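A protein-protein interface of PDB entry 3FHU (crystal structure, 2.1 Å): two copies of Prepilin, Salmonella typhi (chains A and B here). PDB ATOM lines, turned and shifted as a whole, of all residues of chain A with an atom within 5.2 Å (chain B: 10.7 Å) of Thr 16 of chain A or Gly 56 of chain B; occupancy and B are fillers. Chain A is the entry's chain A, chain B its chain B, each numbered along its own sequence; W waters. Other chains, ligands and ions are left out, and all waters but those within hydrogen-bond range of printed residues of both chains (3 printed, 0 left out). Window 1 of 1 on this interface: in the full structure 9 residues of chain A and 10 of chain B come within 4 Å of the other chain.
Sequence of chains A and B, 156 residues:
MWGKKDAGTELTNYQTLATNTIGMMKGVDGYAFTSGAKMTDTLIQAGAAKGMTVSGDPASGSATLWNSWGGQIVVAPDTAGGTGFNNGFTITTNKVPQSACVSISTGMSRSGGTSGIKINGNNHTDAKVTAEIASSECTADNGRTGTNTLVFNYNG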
ATOM      1  N   THR A   9      11.427  -1.096  18.482  1.00  0.00           N
ATOM      2  CA  THR A   9      10.788  -2.401  18.665  1.00  0.00           C
ATOM      3  C   THR A   9      11.844  -3.471  18.855  1.00  0.00           C
ATOM      4  O   THR A   9      11.734  -4.318  19.737  1.00  0.00           O
ATOM      5  CB  THR A   9       9.930  -2.801  17.430  1.00  0.00           C
ATOM      6  OG1 THR A   9       8.899  -1.832  17.235  1.00  0.00           O
ATOM      7  CG2 THR A   9       9.278  -4.169  17.639  1.00  0.00           C
ATOM      8  N   LEU A  11      14.991  -3.117  19.860  1.00  0.00           N
ATOM      9  CA  LEU A  11      15.677  -2.976  21.144  1.00  0.00           C
ATOM     10  C   LEU A  11      14.890  -3.638  22.262  1.00  0.00           C
ATOM     11  O   LEU A  11      15.434  -4.390  23.064  1.00  0.00           O
ATOM     12  CB  LEU A  11      15.889  -1.505  21.494  1.00  0.00           C
ATOM     13  CG  LEU A  11      17.185  -0.875  20.995  1.00  0.00           C
ATOM     14  CD1 LEU A  11      17.134   0.645  21.210  1.00  0.00           C
ATOM     15  CD2 LEU A  11      18.368  -1.495  21.722  1.00  0.00           C
ATOM     16  N   THR A  12      13.597  -3.346  22.300  1.00  0.00           N
ATOM     17  CA  THR A  12      12.714  -3.892  23.312  1.00  0.00           C
ATOM     18  C   THR A  12      12.623  -5.412  23.215  1.00  0.00           C
ATOM     19  O   THR A  12      12.544  -6.099  24.236  1.00  0.00           O
ATOM     20  CB  THR A  12      11.329  -3.249  23.182  1.00  0.00           C
ATOM     21  OG1 THR A  12      11.465  -1.830  23.379  1.00  0.00           O
ATOM     22  CG2 THR A  12      10.348  -3.825  24.206  1.00  0.00           C
ATOM     23  N   ASN A  13      12.642  -5.944  21.994  1.00  0.00           N
ATOM     24  CA  ASN A  13      12.566  -7.391  21.843  1.00  0.00           C
ATOM     25  C   ASN A  13      13.794  -8.065  22.452  1.00  0.00           C
ATOM     26  O   ASN A  13      13.675  -9.054  23.177  1.00  0.00           O
ATOM     27  CB  ASN A  13      12.434  -7.796  20.369  1.00  0.00           C
ATOM     28  CG  ASN A  13      11.020  -7.626  19.840  1.00  0.00           C
ATOM     29  OD1 ASN A  13      10.043  -7.734  20.589  1.00  0.00           O
ATOM     30  ND2 ASN A  13      10.902  -7.390  18.534  1.00  0.00           N
ATOM     31  N   TYR A  14      14.977  -7.530  22.168  1.00  0.00           N
ATOM     32  CA  TYR A  14      16.188  -8.122  22.719  1.00  0.00           C
ATOM     33  C   TYR A  14      16.231  -8.006  24.227  1.00  0.00           C
ATOM     34  O   TYR A  14      16.612  -8.954  24.915  1.00  0.00           O
ATOM     35  CB  TYR A  14      17.435  -7.481  22.113  1.00  0.00           C
ATOM     36  CG  TYR A  14      17.518  -7.737  20.631  1.00  0.00           C
ATOM     37  CD1 TYR A  14      17.357  -9.021  20.129  1.00  0.00           C
ATOM     38  CD2 TYR A  14      17.704  -6.695  19.732  1.00  0.00           C
ATOM     39  CE1 TYR A  14      17.372  -9.264  18.760  1.00  0.00           C
ATOM     40  CE2 TYR A  14      17.726  -6.920  18.364  1.00  0.00           C
ATOM     41  CZ  TYR A  14      17.556  -8.205  17.883  1.00  0.00           C
ATOM     42  OH  TYR A  14      17.579  -8.434  16.529  1.00  0.00           O
ATOM     43  N   GLN A  15      15.819  -6.854  24.743  1.00  0.00           N
ATOM     44  CA  GLN A  15      15.836  -6.632  26.184  1.00  0.00           C
ATOM     45  C   GLN A  15      14.877  -7.547  26.955  1.00  0.00           C
ATOM     46  O   GLN A  15      15.257  -8.135  27.965  1.00  0.00           O
ATOM     47  CB  GLN A  15      15.557  -5.157  26.472  1.00  0.00           C
ATOM     48  CG  GLN A  15      16.716  -4.260  26.025  1.00  0.00           C
ATOM     49  CD  GLN A  15      16.403  -2.781  26.142  1.00  0.00           C
ATOM     50  OE1 GLN A  15      15.409  -2.409  26.738  1.00  0.00           O
ATOM     51  NE2 GLN A  15      17.257  -1.934  25.562  1.00  0.00           N
ATOM     52  N   THR A  16      13.644  -7.671  26.480  1.00  0.00           N
ATOM     53  CA  THR A  16      12.680  -8.538  27.145  1.00  0.00           C
ATOM     54  C   THR A  16      13.078  -9.998  26.933  1.00  0.00           C
ATOM     55  O   THR A  16      12.902 -10.838  27.828  1.00  0.00           O
ATOM     56  CB  THR A  16      11.245  -8.309  26.609  1.00  0.00           C
ATOM     57  OG1 THR A  16      11.223  -8.485  25.184  1.00  0.00           O
ATOM     58  CG2 THR A  16      10.773  -6.890  26.952  1.00  0.00           C
ATOM     59  N   LEU A  17      13.610 -10.310  25.753  1.00  0.00           N
ATOM     60  CA  LEU A  17      14.022 -11.683  25.481  1.00  0.00           C
ATOM     61  C   LEU A  17      15.085 -12.033  26.507  1.00  0.00           C
ATOM     62  O   LEU A  17      15.076 -13.123  27.077  1.00  0.00           O
ATOM     63  CB  LEU A  17      14.595 -11.826  24.061  1.00  0.00           C
ATOM     64  CG  LEU A  17      15.249 -13.162  23.674  1.00  0.00           C
ATOM     65  CD1 LEU A  17      14.339 -14.330  23.999  1.00  0.00           C
ATOM     66  CD2 LEU A  17      15.575 -13.147  22.182  1.00  0.00           C
ATOM     67  N   ALA A  18      15.999 -11.095  26.746  1.00  0.00           N
ATOM     68  CA  ALA A  18      17.059 -11.313  27.721  1.00  0.00           C
ATOM     69  C   ALA A  18      16.446 -11.491  29.111  1.00  0.00           C
ATOM     70  O   ALA A  18      16.802 -12.422  29.840  1.00  0.00           O
ATOM     71  CB  ALA A  18      18.028 -10.138  27.710  1.00  0.00           C
ATOM     72  N   THR A  19      15.527 -10.600  29.481  1.00  0.00           N
ATOM     73  CA  THR A  19      14.870 -10.695  30.783  1.00  0.00           C
ATOM     74  C   THR A  19      14.216 -12.064  30.952  1.00  0.00           C
ATOM     75  O   THR A  19      14.434 -12.744  31.956  1.00  0.00           O
ATOM     76  CB  THR A  19      13.809  -9.581  30.952  1.00  0.00           C
ATOM     77  OG1 THR A  19      14.470  -8.313  30.976  1.00  0.00           O
ATOM     78  CG2 THR A  19      13.018  -9.759  32.248  1.00  0.00           C
ATOM     79  N   ASN A  20      13.428 -12.467  29.958  1.00  0.00           N
ATOM     80  CA  ASN A  20      12.746 -13.755  29.987  1.00  0.00           C
ATOM     81  C   ASN A  20      13.746 -14.906  30.119  1.00  0.00           C
ATOM     82  O   ASN A  20      13.527 -15.848  30.885  1.00  0.00           O
ATOM     83  CB  ASN A  20      11.902 -13.943  28.713  1.00  0.00           C
ATOM     84  CG  ASN A  20      10.772 -12.935  28.604  1.00  0.00           C
ATOM     85  OD1 ASN A  20      10.329 -12.377  29.609  1.00  0.00           O
ATOM     86  ND2 ASN A  20      10.285 -12.718  27.386  1.00  0.00           N
ATOM     87  N   THR A  21      14.839 -14.839  29.367  1.00  0.00           N
ATOM     88  CA  THR A  21      15.837 -15.889  29.449  1.00  0.00           C
ATOM     89  C   THR A  21      16.462 -15.938  30.827  1.00  0.00           C
ATOM     90  O   THR A  21      16.572 -17.014  31.407  1.00  0.00           O
ATOM     91  CB  THR A  21      16.949 -15.711  28.427  1.00  0.00           C
ATOM     92  OG1 THR A  21      16.378 -15.582  27.121  1.00  0.00           O
ATOM     93  CG2 THR A  21      17.856 -16.931  28.446  1.00  0.00           C
ATOM     94  N   ALA A  48       8.785 -16.679  25.303  1.00  0.00           N
ATOM     95  CA  ALA A  48       9.679 -15.582  25.651  1.00  0.00           C
ATOM     96  C   ALA A  48      10.044 -14.662  24.493  1.00  0.00           C
ATOM     97  O   ALA A  48      10.826 -13.732  24.664  1.00  0.00           O
ATOM     98  CB  ALA A  48      10.943 -16.140  26.290  1.00  0.00           C
ATOM     99  N   GLY A  51       7.100 -10.873  20.522  1.00  0.00           N
ATOM    100  CA  GLY A  51       7.202  -9.756  19.599  1.00  0.00           C
ATOM    101  C   GLY A  51       8.057 -10.005  18.375  1.00  0.00           C
ATOM    102  O   GLY A  51       8.071  -9.193  17.455  1.00  0.00           O
ATOM    103  N   ALA B  37      -0.552   1.013  25.916  1.00  0.00           N
ATOM    104  CA  ALA B  37       0.761   0.641  25.416  1.00  0.00           C
ATOM    105  C   ALA B  37       1.872   1.348  26.184  1.00  0.00           C
ATOM    106  O   ALA B  37       2.850   0.730  26.592  1.00  0.00           O
ATOM    107  CB  ALA B  37       0.864   0.965  23.925  1.00  0.00           C
ATOM    108  N   THR B  40       1.796   0.513  30.203  1.00  0.00           N
ATOM    109  CA  THR B  40       2.343  -0.819  30.466  1.00  0.00           C
ATOM    110  C   THR B  40       3.861  -0.790  30.275  1.00  0.00           C
ATOM    111  O   THR B  40       4.614  -1.325  31.084  1.00  0.00           O
ATOM    112  CB  THR B  40       1.689  -1.856  29.522  1.00  0.00           C
ATOM    113  OG1 THR B  40       0.263  -1.817  29.709  1.00  0.00           O
ATOM    114  CG2 THR B  40       2.195  -3.274  29.821  1.00  0.00           C
ATOM    115  N   ASP B  41       4.302  -0.143  29.200  1.00  0.00           N
ATOM    116  CA  ASP B  41       5.730  -0.020  28.931  1.00  0.00           C
ATOM    117  C   ASP B  41       6.428   0.606  30.133  1.00  0.00           C
ATOM    118  O   ASP B  41       7.417   0.081  30.633  1.00  0.00           O
ATOM    119  CB  ASP B  41       5.973   0.865  27.710  1.00  0.00           C
ATOM    120  CG  ASP B  41       7.453   1.099  27.448  1.00  0.00           C
ATOM    121  OD1 ASP B  41       8.146   0.154  27.029  1.00  0.00           O
ATOM    122  OD2 ASP B  41       7.924   2.225  27.678  1.00  0.00           O
ATOM    123  N   THR B  42       5.900   1.732  30.593  1.00  0.00           N
ATOM    124  CA  THR B  42       6.499   2.440  31.718  1.00  0.00           C
ATOM    125  C   THR B  42       6.566   1.570  32.983  1.00  0.00           C
ATOM    126  O   THR B  42       7.572   1.567  33.692  1.00  0.00           O
ATOM    127  CB  THR B  42       5.727   3.744  31.968  1.00  0.00           C
ATOM    128  OG1 THR B  42       5.754   4.530  30.765  1.00  0.00           O
ATOM    129  CG2 THR B  42       6.358   4.543  33.084  1.00  0.00           C
ATOM    130  N   LEU B  43       5.498   0.821  33.250  1.00  0.00           N
ATOM    131  CA  LEU B  43       5.459  -0.073  34.402  1.00  0.00           C
ATOM    132  C   LEU B  43       6.600  -1.072  34.301  1.00  0.00           C
ATOM    133  O   LEU B  43       7.345  -1.299  35.265  1.00  0.00           O
ATOM    134  CB  LEU B  43       4.153  -0.859  34.424  1.00  0.00           C
ATOM    135  CG  LEU B  43       2.919  -0.185  34.998  1.00  0.00           C
ATOM    136  CD1 LEU B  43       1.816  -1.235  35.076  1.00  0.00           C
ATOM    137  CD2 LEU B  43       3.230   0.370  36.390  1.00  0.00           C
ATOM    138  N   ILE B  44       6.702  -1.681  33.122  1.00  0.00           N
ATOM    139  CA  ILE B  44       7.725  -2.676  32.836  1.00  0.00           C
ATOM    140  C   ILE B  44       9.114  -2.068  33.030  1.00  0.00           C
ATOM    141  O   ILE B  44       9.968  -2.655  33.696  1.00  0.00           O
ATOM    142  CB  ILE B  44       7.533  -3.242  31.389  1.00  0.00           C
ATOM    143  CG1 ILE B  44       6.210  -4.025  31.320  1.00  0.00           C
ATOM    144  CG2 ILE B  44       8.678  -4.170  31.006  1.00  0.00           C
ATOM    145  CD1 ILE B  44       5.911  -4.646  29.956  1.00  0.00           C
ATOM    146  N   GLN B  45       9.345  -0.882  32.474  1.00  0.00           N
ATOM    147  CA  GLN B  45      10.649  -0.242  32.636  1.00  0.00           C
ATOM    148  C   GLN B  45      10.971  -0.013  34.106  1.00  0.00           C
ATOM    149  O   GLN B  45      12.128  -0.086  34.521  1.00  0.00           O
ATOM    150  CB  GLN B  45      10.689   1.107  31.909  1.00  0.00           C
ATOM    151  CG  GLN B  45      10.488   1.027  30.402  1.00  0.00           C
ATOM    152  CD  GLN B  45      11.341  -0.033  29.762  1.00  0.00           C
ATOM    153  OE1 GLN B  45      12.523  -0.182  30.093  1.00  0.00           O
ATOM    154  NE2 GLN B  45      10.758  -0.781  28.830  1.00  0.00           N
ATOM    155  N   ALA B  49       7.181  -5.636  36.376  1.00  0.00           N
ATOM    156  CA  ALA B  49       6.741  -6.902  35.792  1.00  0.00           C
ATOM    157  C   ALA B  49       7.720  -8.068  35.850  1.00  0.00           C
ATOM    158  O   ALA B  49       7.481  -9.117  35.238  1.00  0.00           O
ATOM    159  CB  ALA B  49       6.304  -6.658  34.346  1.00  0.00           C
ATOM    160  N   LYS B  50       8.806  -7.893  36.596  1.00  0.00           N
ATOM    161  CA  LYS B  50       9.808  -8.934  36.754  1.00  0.00           C
ATOM    162  C   LYS B  50       9.153 -10.239  37.181  1.00  0.00           C
ATOM    163  O   LYS B  50       8.392 -10.263  38.144  1.00  0.00           O
ATOM    164  CB  LYS B  50      10.831  -8.526  37.813  1.00  0.00           C
ATOM    165  CG  LYS B  50      11.549  -7.227  37.521  1.00  0.00           C
ATOM    166  CD  LYS B  50      12.336  -7.330  36.236  1.00  0.00           C
ATOM    167  CE  LYS B  50      13.039  -6.011  35.932  1.00  0.00           C
ATOM    168  NZ  LYS B  50      13.737  -6.116  34.622  1.00  0.00           N
ATOM    169  N   GLY B  51       9.458 -11.316  36.459  1.00  0.00           N
ATOM    170  CA  GLY B  51       8.910 -12.620  36.770  1.00  0.00           C
ATOM    171  C   GLY B  51       7.715 -12.945  35.899  1.00  0.00           C
ATOM    172  O   GLY B  51       7.190 -14.052  35.929  1.00  0.00           O
ATOM    173  N   MET B  52       7.263 -11.957  35.139  1.00  0.00           N
ATOM    174  CA  MET B  52       6.139 -12.147  34.249  1.00  0.00           C
ATOM    175  C   MET B  52       6.696 -12.052  32.851  1.00  0.00           C
ATOM    176  O   MET B  52       7.654 -11.320  32.611  1.00  0.00           O
ATOM    177  CB  MET B  52       5.094 -11.056  34.468  1.00  0.00           C
ATOM    178  CG  MET B  52       4.507 -11.065  35.866  1.00  0.00           C
ATOM    179  SD  MET B  52       3.237  -9.833  35.986  1.00  0.00           S
ATOM    180  CE  MET B  52       1.920 -10.648  35.202  1.00  0.00           C
ATOM    181  N   THR B  53       6.094 -12.788  31.933  1.00  0.00           N
ATOM    182  CA  THR B  53       6.547 -12.798  30.552  1.00  0.00           C
ATOM    183  C   THR B  53       6.282 -11.470  29.875  1.00  0.00           C
ATOM    184  O   THR B  53       5.152 -10.995  29.840  1.00  0.00           O
ATOM    185  CB  THR B  53       5.840 -13.908  29.746  1.00  0.00           C
ATOM    186  OG1 THR B  53       6.222 -15.181  30.268  1.00  0.00           O
ATOM    187  CG2 THR B  53       6.224 -13.844  28.267  1.00  0.00           C
ATOM    188  N   VAL B  54       7.350 -10.883  29.348  1.00  0.00           N
ATOM    189  CA  VAL B  54       7.294  -9.627  28.641  1.00  0.00           C
ATOM    190  C   VAL B  54       7.866  -9.808  27.230  1.00  0.00           C
ATOM    191  O   VAL B  54       8.530 -10.799  26.935  1.00  0.00           O
ATOM    192  CB  VAL B  54       8.118  -8.541  29.375  1.00  0.00           C
ATOM    193  CG1 VAL B  54       7.418  -8.147  30.674  1.00  0.00           C
ATOM    194  CG2 VAL B  54       9.525  -9.073  29.709  1.00  0.00           C
ATOM    195  N   SER B  55       7.592  -8.843  26.362  1.00  0.00           N
ATOM    196  CA  SER B  55       8.111  -8.847  24.998  1.00  0.00           C
ATOM    197  C   SER B  55       7.970  -7.424  24.469  1.00  0.00           C
ATOM    198  O   SER B  55       7.679  -6.512  25.230  1.00  0.00           O
ATOM    199  CB  SER B  55       7.342  -9.816  24.101  1.00  0.00           C
ATOM    200  OG  SER B  55       8.053 -10.012  22.886  1.00  0.00           O
ATOM    201  N   GLY B  56       8.181  -7.229  23.176  1.00  0.00           N
ATOM    202  CA  GLY B  56       8.077  -5.891  22.623  1.00  0.00           C
ATOM    203  C   GLY B  56       6.980  -5.778  21.583  1.00  0.00           C
ATOM    204  O   GLY B  56       6.730  -6.709  20.836  1.00  0.00           O
ATOM    205  N   ASP B  57       6.337  -4.620  21.531  1.00  0.00           N
ATOM    206  CA  ASP B  57       5.250  -4.376  20.597  1.00  0.00           C
ATOM    207  C   ASP B  57       5.731  -3.697  19.311  1.00  0.00           C
ATOM    208  O   ASP B  57       6.237  -2.578  19.344  1.00  0.00           O
ATOM    209  CB  ASP B  57       4.184  -3.530  21.295  1.00  0.00           C
ATOM    210  CG  ASP B  57       3.279  -2.823  20.330  1.00  0.00           C
ATOM    211  OD1 ASP B  57       2.950  -3.418  19.284  1.00  0.00           O
ATOM    212  OD2 ASP B  57       2.903  -1.664  20.632  1.00  0.00           O
ATOM    213  N   PRO B  58       5.557  -4.370  18.158  1.00  0.00           N
ATOM    214  CA  PRO B  58       5.959  -3.884  16.832  1.00  0.00           C
ATOM    215  C   PRO B  58       5.368  -2.542  16.406  1.00  0.00           C
ATOM    216  O   PRO B  58       5.986  -1.801  15.647  1.00  0.00           O
ATOM    217  CB  PRO B  58       5.506  -5.016  15.897  1.00  0.00           C
ATOM    218  CG  PRO B  58       5.513  -6.193  16.749  1.00  0.00           C
ATOM    219  CD  PRO B  58       4.903  -5.682  18.027  1.00  0.00           C
ATOM    220  N   ALA B  59       4.171  -2.231  16.889  1.00  0.00           N
ATOM    221  CA  ALA B  59       3.505  -0.989  16.510  1.00  0.00           C
ATOM    222  C   ALA B  59       4.052   0.264  17.200  1.00  0.00           C
ATOM    223  O   ALA B  59       3.953   1.371  16.663  1.00  0.00           O
ATOM    224  CB  ALA B  59       1.996  -1.116  16.771  1.00  0.00           C
ATOM    225  N   SER B  60       4.644   0.105  18.377  1.00  0.00           N
ATOM    226  CA  SER B  60       5.145   1.270  19.105  1.00  0.00           C
ATOM    227  C   SER B  60       6.554   1.144  19.671  1.00  0.00           C
ATOM    228  O   SER B  60       7.165   2.151  20.032  1.00  0.00           O
ATOM    229  CB  SER B  60       4.178   1.603  20.243  1.00  0.00           C
ATOM    230  OG  SER B  60       4.084   0.513  21.143  1.00  0.00           O
ATOM    231  N   GLY B  61       7.074  -0.076  19.744  1.00  0.00           N
ATOM    232  CA  GLY B  61       8.395  -0.270  20.317  1.00  0.00           C
ATOM    233  C   GLY B  61       8.262  -0.359  21.833  1.00  0.00           C
ATOM    234  O   GLY B  61       9.242  -0.461  22.570  1.00  0.00           O
ATOM    235  N   SER B  62       7.024  -0.319  22.308  1.00  0.00           N
ATOM    236  CA  SER B  62       6.769  -0.413  23.741  1.00  0.00           C
ATOM    237  C   SER B  62       6.812  -1.874  24.187  1.00  0.00           C
ATOM    238  O   SER B  62       6.558  -2.784  23.393  1.00  0.00           O
ATOM    239  CB  SER B  62       5.400   0.182  24.070  1.00  0.00           C
ATOM    240  OG  SER B  62       5.368   1.559  23.721  1.00  0.00           O
ATOM    241  N   ALA B  63       7.140  -2.090  25.457  1.00  0.00           N
ATOM    242  CA  ALA B  63       7.199  -3.437  26.008  1.00  0.00           C
ATOM    243  C   ALA B  63       5.771  -3.878  26.358  1.00  0.00           C
ATOM    244  O   ALA B  63       4.983  -3.080  26.852  1.00  0.00           O
ATOM    245  CB  ALA B  63       8.076  -3.462  27.264  1.00  0.00           C
ATOM    246  N   THR B  64       5.466  -5.145  26.083  1.00  0.00           N
ATOM    247  CA  THR B  64       4.162  -5.745  26.346  1.00  0.00           C
ATOM    248  C   THR B  64       4.249  -6.763  27.494  1.00  0.00           C
ATOM    249  O   THR B  64       5.325  -7.279  27.810  1.00  0.00           O
ATOM    250  CB  THR B  64       3.627  -6.473  25.102  1.00  0.00           C
ATOM    251  OG1 THR B  64       4.565  -7.488  24.714  1.00  0.00           O
ATOM    252  CG2 THR B  64       3.438  -5.496  23.955  1.00  0.00           C
ATOM    253  N   LEU B  65       3.096  -7.059  28.088  1.00  0.00           N
ATOM    254  CA  LEU B  65       2.992  -7.978  29.223  1.00  0.00           C
ATOM    255  C   LEU B  65       2.030  -9.129  28.891  1.00  0.00           C
ATOM    256  O   LEU B  65       1.029  -8.922  28.217  1.00  0.00           O
ATOM    257  CB  LEU B  65       2.464  -7.204  30.436  1.00  0.00           C
ATOM    258  CG  LEU B  65       2.608  -7.795  31.833  1.00  0.00           C
ATOM    259  CD1 LEU B  65       4.094  -7.986  32.165  1.00  0.00           C
ATOM    260  CD2 LEU B  65       1.964  -6.856  32.840  1.00  0.00           C
ATOM    261  N   TRP B  66       2.350 -10.330  29.362  1.00  0.00           N
ATOM    262  CA  TRP B  66       1.498 -11.490  29.130  1.00  0.00           C
ATOM    263  C   TRP B  66       1.187 -12.203  30.440  1.00  0.00           C
ATOM    264  O   TRP B  66       1.954 -12.119  31.399  1.00  0.00           O
ATOM    265  CB  TRP B  66       2.166 -12.457  28.150  1.00  0.00           C
ATOM    266  CG  TRP B  66       2.601 -11.808  26.872  1.00  0.00           C
ATOM    267  CD1 TRP B  66       3.852 -11.357  26.567  1.00  0.00           C
ATOM    268  CD2 TRP B  66       1.787 -11.537  25.725  1.00  0.00           C
ATOM    269  NE1 TRP B  66       3.867 -10.822  25.302  1.00  0.00           N
ATOM    270  CE2 TRP B  66       2.611 -10.921  24.763  1.00  0.00           C
ATOM    271  CE3 TRP B  66       0.440 -11.756  25.418  1.00  0.00           C
ATOM    272  CZ2 TRP B  66       2.134 -10.521  23.517  1.00  0.00           C
ATOM    273  CZ3 TRP B  66      -0.032 -11.357  24.180  1.00  0.00           C
ATOM    274  CH2 TRP B  66       0.813 -10.747  23.245  1.00  0.00           C
ATOM    275  N   GLN B  72      -2.715 -11.591  26.672  1.00  0.00           N
ATOM    276  CA  GLN B  72      -2.043 -10.332  26.953  1.00  0.00           C
ATOM    277  C   GLN B  72      -2.632  -9.658  28.180  1.00  0.00           C
ATOM    278  O   GLN B  72      -3.806  -9.836  28.492  1.00  0.00           O
ATOM    279  CB  GLN B  72      -2.132  -9.380  25.750  1.00  0.00           C
ATOM    280  CG  GLN B  72      -1.371  -8.062  25.936  1.00  0.00           C
ATOM    281  CD  GLN B  72      -1.138  -7.314  24.627  1.00  0.00           C
ATOM    282  OE1 GLN B  72      -1.858  -7.499  23.656  1.00  0.00           O
ATOM    283  NE2 GLN B  72      -0.131  -6.448  24.609  1.00  0.00           N
HETATM  284  O   HOH W   1       7.677 -12.910  24.998  1.00  0.00           O
HETATM  285  O   HOH W   2      10.053 -12.715  32.615  1.00  0.00           O
HETATM  286  O   HOH W   3      10.900 -10.988  23.871  1.00  0.00           O
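Water W2 lies within hydrogen-bond range of the backbone carbonyl oxygen of Met 52 of chain B (2.8 Å) and the side-chain amide oxygen of Asn 20 of chain A (3.0 Å). Water W3 lies within hydrogen-bond range of the side-chain hydroxyl (OG1) of Thr 16 of chain A (2.8 Å), the backbone carbonyl oxygen (O) of Ala 48 of chain A (2.9 Å), the side-chain hydroxyl (OG) of Ser 55 of chain B (3.2 Å), the backbone NH (N) of Leu 17 of chain A (3.4 Å) and the backbone carbonyl oxygen (O) of Asn 13 of chain A (3.5 Å). Water W1 lies within hydrogen-bond range of the backbone carbonyl oxygen (O) of Val 54 of chain B and the backbone carbonyl oxygen (O) of Ala 48 of chain A.
Position printed for both chains: 51.
Of the 26 printed residues of chain B, 8 touch a printed residue of chain A. Printed residues of chain B that touch a printed residue of chain A: Thr 53, Val 54, Ser 55, Gly 56, Asp 57, Pro 58, Gly 61 and Ala 63. Among the printed residues, 16 pairs touch across the chains. Among the printed residues, no Asp or Glu carboxylate lies within 4 Å of a Lys or Arg side-chain nitrogen of the other chain.
The backbone carbonyl oxygen (O) of Asp 57 of chain B sits at hydrogen-bond distance from the side-chain hydroxyl (OG1) of Thr 9 of chain A (3.5 Å). OG1 of Thr 9 of chain A is in hydrogen-bond range of O of Pro 58 of chain B (3.3 Å). The side-chain hydroxyl (OG1) of Thr 12 of chain A is in hydrogen-bond range of the backbone carbonyl oxygen (O) of Gly 61 of chain B (2.7 Å). The side-chain amide oxygen of Asn 13 of chain A lies within hydrogen-bond range of the backbone NH of Gly 56 of chain B, at 3.2 Å. The side-chain amide nitrogen of Asn 20 of chain A sits at hydrogen-bond distance from the backbone carbonyl oxygen of Val 54 of chain B (2.6 Å). N of Gly 51 of chain A is in hydrogen-bond range of OG of Ser 55 of chain B (2.7 Å).
Thr 16 of chain A touches three residues of chain B. Asn 13 of chain A touches just these residues of chain B: Ser 55 (3.8 Å) and Gly 56 (3.2 Å). Leu 17 of chain A touches none of the printed residues of chain B. No residue of chain B comes within 4 Å of Thr 19 of chain A. Of the printed residues of chain A, Asp 57 of chain B touches Thr 9. Of the printed residues of chain A, Ser 55 of chain B touches Thr 12, Asn 13, Thr 16 and Gly 51. Printed residues of chain B within 4 Å of Thr 12 of chain A: Ser 55 (3.9 Å), Gly 56 (3.5 Å), Gly 61 (2.7 Å) and Ala 63 (3.6 Å). Of the printed residues of chain A, Ala 63 of chain B touches Thr 12. Printed residues of chain A within 4 Å of Pro 58 of chain B: Thr 9. Gln 72 of chain B touches none of the printed residues of chain A. The nearest residue of chain A that does not touch Gly 56 of chain B is Thr 9 of chain A (4.8 Å). The nearest printed residue of chain B that does not touch Gly 51 of chain A is Pro 58 of chain B (4.01 Å).
Among the printed residues, pairs that only touch across the chains: Thr 16 of chain A with Ser 55 of chain B (3.1 Å), Gly 51 of chain A with Gly 56 of chain B (3.3 Å), Thr 12 of chain A with Gly 56 of chain B (3.5 Å), Thr 9 of chain A with Gly 61 of chain B (3.5 Å), Thr 16 of chain A with Val 54 of chain B (3.6 Å), Thr 12 of chain A with Ala 63 of chain B (3.6 Å), Asn 13 of chain A with Ser 55 of chain B (3.8 Å), Thr 16 of chain A with Gly 56 of chain B (3.9 Å), Asn 20 of chain A with Thr 53 of chain B (3.9 Å) and Thr 12 of chain A with Ser 55 of chain B (3.9 Å).
The backbone carbonyl oxygen (O) of Thr 9 of chain A lies close to the side-chain amide nitrogen (ND2) of Asn 13 of chain A (3.4 Å). O of Thr 12 of chain A lies within hydrogen-bond range of OG1 of Thr 16 of chain A, at 2.9 Å. O of Asn 13 of chain A sits at hydrogen-bond distance from OG1 of Thr 16 of chain A (3.2 Å). The backbone NH of Ala 63 of chain B is in hydrogen-bond range of the side-chain carboxylate of Asp 41 of chain B. OD1 of Asp 57 of chain B lies within hydrogen-bond range of N of Ala 59 of chain B (2.9 Å). O of Ser 62 of chain B lies within hydrogen-bond range of N of Asp 57 of chain B, 2.6 Å away.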
